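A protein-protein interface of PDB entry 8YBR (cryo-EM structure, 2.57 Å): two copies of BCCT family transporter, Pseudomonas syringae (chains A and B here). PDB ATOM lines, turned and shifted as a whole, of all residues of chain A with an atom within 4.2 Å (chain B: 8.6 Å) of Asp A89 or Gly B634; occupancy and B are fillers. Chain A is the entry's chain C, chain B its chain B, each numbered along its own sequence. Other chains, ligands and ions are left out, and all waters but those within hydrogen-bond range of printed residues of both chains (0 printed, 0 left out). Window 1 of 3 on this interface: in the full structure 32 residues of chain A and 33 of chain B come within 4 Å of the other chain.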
ATOM      1  N   ALA A  88      -2.523 -18.914   1.178  1.00  0.00           N
ATOM      2  CA  ALA A  88      -3.298 -18.002   2.002  1.00  0.00           C
ATOM      3  C   ALA A  88      -4.299 -17.236   1.144  1.00  0.00           C
ATOM      4  O   ALA A  88      -4.182 -17.171  -0.080  1.00  0.00           O
ATOM      5  CB  ALA A  88      -2.382 -17.030   2.743  1.00  0.00           C
ATOM      6  N   ASP A  89      -5.289 -16.640   1.809  1.00  0.00           N
ATOM      7  CA  ASP A  89      -6.372 -15.959   1.107  1.00  0.00           C
ATOM      8  C   ASP A  89      -5.928 -14.687   0.400  1.00  0.00           C
ATOM      9  O   ASP A  89      -6.683 -14.168  -0.427  1.00  0.00           O
ATOM     10  CB  ASP A  89      -7.506 -15.636   2.077  1.00  0.00           C
ATOM     11  CG  ASP A  89      -8.306 -16.860   2.461  1.00  0.00           C
ATOM     12  OD1 ASP A  89      -8.412 -17.785   1.627  1.00  0.00           O
ATOM     13  OD2 ASP A  89      -8.828 -16.901   3.594  1.00  0.00           O
ATOM     14  N   HIS A  90      -4.738 -14.170   0.697  1.00  0.00           N
ATOM     15  CA  HIS A  90      -4.212 -12.995   0.017  1.00  0.00           C
ATOM     16  C   HIS A  90      -3.114 -13.349  -0.977  1.00  0.00           C
ATOM     17  O   HIS A  90      -2.374 -12.465  -1.419  1.00  0.00           O
ATOM     18  CB  HIS A  90      -3.701 -11.979   1.038  1.00  0.00           C
ATOM     19  CG  HIS A  90      -4.777 -11.134   1.640  1.00  0.00           C
ATOM     20  ND1 HIS A  90      -6.001 -10.944   1.036  1.00  0.00           N
ATOM     21  CD2 HIS A  90      -4.814 -10.424   2.791  1.00  0.00           C
ATOM     22  CE1 HIS A  90      -6.747 -10.156   1.789  1.00  0.00           C
ATOM     23  NE2 HIS A  90      -6.049  -9.827   2.862  1.00  0.00           N
ATOM     24  N   ASP A  91      -2.994 -14.624  -1.338  1.00  0.00           N
ATOM     25  CA  ASP A  91      -1.997 -15.074  -2.299  1.00  0.00           C
ATOM     26  C   ASP A  91      -2.540 -14.969  -3.716  1.00  0.00           C
ATOM     27  O   ASP A  91      -3.736 -15.162  -3.954  1.00  0.00           O
ATOM     28  CB  ASP A  91      -1.578 -16.516  -2.015  1.00  0.00           C
ATOM     29  CG  ASP A  91      -0.467 -16.611  -0.996  1.00  0.00           C
ATOM     30  OD1 ASP A  91       0.186 -15.581  -0.731  1.00  0.00           O
ATOM     31  OD2 ASP A  91      -0.235 -17.715  -0.467  1.00  0.00           O
ATOM     32  N   GLN A 515     -16.699 -22.016  12.530  1.00  0.00           N
ATOM     33  CA  GLN A 515     -16.436 -20.590  12.400  1.00  0.00           C
ATOM     34  C   GLN A 515     -17.685 -19.783  12.085  1.00  0.00           C
ATOM     35  O   GLN A 515     -17.698 -18.575  12.333  1.00  0.00           O
ATOM     36  CB  GLN A 515     -15.379 -20.312  11.323  1.00  0.00           C
ATOM     37  CG  GLN A 515     -15.843 -20.503   9.891  1.00  0.00           C
ATOM     38  CD  GLN A 515     -14.732 -20.240   8.887  1.00  0.00           C
ATOM     39  OE1 GLN A 515     -13.608 -19.911   9.263  1.00  0.00           O
ATOM     40  NE2 GLN A 515     -15.047 -20.367   7.604  1.00  0.00           N
ATOM     41  N   TYR B 517     -19.900 -10.682   2.736  1.00  0.00           N
ATOM     42  CA  TYR B 517     -18.762 -10.151   3.476  1.00  0.00           C
ATOM     43  C   TYR B 517     -19.009  -8.747   4.008  1.00  0.00           C
ATOM     44  O   TYR B 517     -18.258  -8.288   4.872  1.00  0.00           O
ATOM     45  CB  TYR B 517     -17.519 -10.146   2.588  1.00  0.00           C
ATOM     46  CG  TYR B 517     -16.757 -11.452   2.583  1.00  0.00           C
ATOM     47  CD1 TYR B 517     -17.394 -12.650   2.300  1.00  0.00           C
ATOM     48  CD2 TYR B 517     -15.399 -11.484   2.862  1.00  0.00           C
ATOM     49  CE1 TYR B 517     -16.702 -13.843   2.294  1.00  0.00           C
ATOM     50  CE2 TYR B 517     -14.698 -12.671   2.860  1.00  0.00           C
ATOM     51  CZ  TYR B 517     -15.354 -13.847   2.574  1.00  0.00           C
ATOM     52  OH  TYR B 517     -14.656 -15.033   2.571  1.00  0.00           O
ATOM     53  N   HIS B 630      -6.683  -7.597   9.649  1.00  0.00           N
ATOM     54  CA  HIS B 630      -6.670  -8.984   9.222  1.00  0.00           C
ATOM     55  C   HIS B 630      -6.616  -9.901  10.435  1.00  0.00           C
ATOM     56  O   HIS B 630      -6.137  -9.521  11.505  1.00  0.00           O
ATOM     57  CB  HIS B 630      -5.488  -9.260   8.290  1.00  0.00           C
ATOM     58  CG  HIS B 630      -5.412  -8.321   7.127  1.00  0.00           C
ATOM     59  ND1 HIS B 630      -5.949  -8.617   5.894  1.00  0.00           N
ATOM     60  CD2 HIS B 630      -4.875  -7.083   7.018  1.00  0.00           C
ATOM     61  CE1 HIS B 630      -5.742  -7.603   5.072  1.00  0.00           C
ATOM     62  NE2 HIS B 630      -5.093  -6.660   5.730  1.00  0.00           N
ATOM     63  N   LEU B 631      -7.121 -11.115  10.255  1.00  0.00           N
ATOM     64  CA  LEU B 631      -7.215 -12.102  11.324  1.00  0.00           C
ATOM     65  C   LEU B 631      -6.822 -13.448  10.725  1.00  0.00           C
ATOM     66  O   LEU B 631      -6.231 -13.521   9.643  1.00  0.00           O
ATOM     67  CB  LEU B 631      -8.626 -12.111  11.936  1.00  0.00           C
ATOM     68  CG  LEU B 631      -9.199 -10.798  12.470  1.00  0.00           C
ATOM     69  CD1 LEU B 631     -10.710 -10.841  12.470  1.00  0.00           C
ATOM     70  CD2 LEU B 631      -8.682 -10.513  13.863  1.00  0.00           C
ATOM     71  N   SER B 632      -7.139 -14.531  11.427  1.00  0.00           N
ATOM     72  CA  SER B 632      -6.890 -15.850  10.874  1.00  0.00           C
ATOM     73  C   SER B 632      -7.800 -16.100   9.671  1.00  0.00           C
ATOM     74  O   SER B 632      -8.684 -15.301   9.346  1.00  0.00           O
ATOM     75  CB  SER B 632      -7.089 -16.926  11.940  1.00  0.00           C
ATOM     76  OG  SER B 632      -6.124 -16.798  12.970  1.00  0.00           O
ATOM     77  N   GLU B 633      -7.572 -17.229   9.009  1.00  0.00           N
ATOM     78  CA  GLU B 633      -8.238 -17.510   7.746  1.00  0.00           C
ATOM     79  C   GLU B 633      -9.748 -17.622   7.943  1.00  0.00           C
ATOM     80  O   GLU B 633     -10.238 -18.126   8.956  1.00  0.00           O
ATOM     81  CB  GLU B 633      -7.686 -18.794   7.123  1.00  0.00           C
ATOM     82  CG  GLU B 633      -6.236 -18.682   6.674  1.00  0.00           C
ATOM     83  CD  GLU B 633      -5.684 -19.984   6.127  1.00  0.00           C
ATOM     84  OE1 GLU B 633      -6.361 -21.021   6.268  1.00  0.00           O
ATOM     85  OE2 GLU B 633      -4.570 -19.970   5.558  1.00  0.00           O
ATOM     86  N   GLY B 634     -10.489 -17.152   6.941  1.00  0.00           N
ATOM     87  CA  GLY B 634     -11.933 -17.078   7.037  1.00  0.00           C
ATOM     88  C   GLY B 634     -12.405 -15.958   7.943  1.00  0.00           C
ATOM     89  O   GLY B 634     -12.937 -16.209   9.028  1.00  0.00           O
ATOM     90  N   SER B 635     -12.205 -14.718   7.511  1.00  0.00           N
ATOM     91  CA  SER B 635     -12.587 -13.545   8.287  1.00  0.00           C
ATOM     92  C   SER B 635     -12.919 -12.415   7.317  1.00  0.00           C
ATOM     93  O   SER B 635     -12.922 -12.604   6.096  1.00  0.00           O
ATOM     94  CB  SER B 635     -11.475 -13.157   9.266  1.00  0.00           C
ATOM     95  OG  SER B 635     -10.479 -12.387   8.619  1.00  0.00           O
ATOM     96  N   GLN B 636     -13.212 -11.236   7.865  1.00  0.00           N
ATOM     97  CA  GLN B 636     -13.526 -10.056   7.070  1.00  0.00           C
ATOM     98  C   GLN B 636     -12.491  -8.975   7.342  1.00  0.00           C
ATOM     99  O   GLN B 636     -11.804  -8.986   8.365  1.00  0.00           O
ATOM    100  CB  GLN B 636     -14.931  -9.522   7.374  1.00  0.00           C
ATOM    101  CG  GLN B 636     -16.065 -10.368   6.817  1.00  0.00           C
ATOM    102  CD  GLN B 636     -16.240 -11.676   7.560  1.00  0.00           C
ATOM    103  OE1 GLN B 636     -16.137 -12.755   6.976  1.00  0.00           O
ATOM    104  NE2 GLN B 636     -16.506 -11.586   8.857  1.00  0.00           N
ATOM    105  N   ASP B 637     -12.389  -8.029   6.412  1.00  0.00           N
ATOM    106  CA  ASP B 637     -11.428  -6.937   6.494  1.00  0.00           C
ATOM    107  C   ASP B 637     -12.169  -5.609   6.555  1.00  0.00           C
ATOM    108  O   ASP B 637     -13.077  -5.366   5.756  1.00  0.00           O
ATOM    109  CB  ASP B 637     -10.478  -6.953   5.296  1.00  0.00           C
ATOM    110  CG  ASP B 637      -9.607  -8.192   5.261  1.00  0.00           C
ATOM    111  OD1 ASP B 637      -9.363  -8.780   6.334  1.00  0.00           O
ATOM    112  OD2 ASP B 637      -9.157  -8.577   4.162  1.00  0.00           O
ATOM    113  N   GLN B 655     -13.198  -9.409  19.569  1.00  0.00           N
ATOM    114  CA  GLN B 655     -12.617 -10.327  18.600  1.00  0.00           C
ATOM    115  C   GLN B 655     -11.846 -11.444  19.280  1.00  0.00           C
ATOM    116  O   GLN B 655     -11.683 -12.522  18.698  1.00  0.00           O
ATOM    117  CB  GLN B 655     -11.694  -9.579  17.635  1.00  0.00           C
ATOM    118  CG  GLN B 655     -12.409  -8.612  16.703  1.00  0.00           C
ATOM    119  CD  GLN B 655     -13.153  -9.309  15.584  1.00  0.00           C
ATOM    120  OE1 GLN B 655     -13.065 -10.524  15.423  1.00  0.00           O
ATOM    121  NE2 GLN B 655     -13.892  -8.538  14.803  1.00  0.00           N
ATOM    122  N   PHE B 662     -14.627 -20.142  19.283  1.00  0.00           N
ATOM    123  CA  PHE B 662     -14.202 -20.989  18.175  1.00  0.00           C
ATOM    124  C   PHE B 662     -13.385 -22.172  18.677  1.00  0.00           C
ATOM    125  O   PHE B 662     -13.590 -23.310  18.243  1.00  0.00           O
ATOM    126  CB  PHE B 662     -13.404 -20.164  17.168  1.00  0.00           C
ATOM    127  CG  PHE B 662     -12.708 -20.983  16.123  1.00  0.00           C
ATOM    128  CD1 PHE B 662     -11.357 -21.254  16.223  1.00  0.00           C
ATOM    129  CD2 PHE B 662     -13.401 -21.472  15.034  1.00  0.00           C
ATOM    130  CE1 PHE B 662     -10.716 -22.006  15.264  1.00  0.00           C
ATOM    131  CE2 PHE B 662     -12.760 -22.222  14.072  1.00  0.00           C
ATOM    132  CZ  PHE B 662     -11.420 -22.489  14.189  1.00  0.00           C
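ND1 of His B630 lies close to NE2 of His A90, at 3.3 Å.
The side-chain carboxylate (OD1) of Asp B637 lies within hydrogen-bond range of a ring nitrogen (ND1) of His B630, at 3.4 Å.
Among the printed residues, merely in contact across the chains: His A90 with Asp B637, Asp A89 with Gly B634, Gln A515 with Gly B634 and Gln A515 with Glu B633.
Asp A89 touches one residue of chain B. Of chain A, only Asp A89 and Gln A515 come within 4 Å of Gly B634. Of the printed residues of chain A, Glu B633 touches Gln A515 (3.8 Å). Printed residues of chain A within 4 Å of His B630: His A90. Of the printed residues of chain B, His A90 touches His B630 (3.2 Å) and Asp B637 (3.6 Å). Of the printed residues of chain B, Gln A515 touches Glu B633 and Gly B634. Of the printed residues of chain A, Asp B637 touches His A90. Gln B655 touches none of the printed residues of chain A.
Printed residues of chain B that touch a printed residue of chain A: His B630, Glu B633, Gly B634 and Asp B637. Hydrophobic or aromatic side chains of chain B within 4 Å of the printed part of chain A: His B630. Of the 5 printed residues of chain A, 3 touch a printed residue of chain B. Hydrophobic or aromatic side chains of chain A that line the printed part of chain B: His A90.
No position is printed for both chains. Of the 5 pairs that touch across the chains among the printed residues, none has its exchanged pair printed and touching as well.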
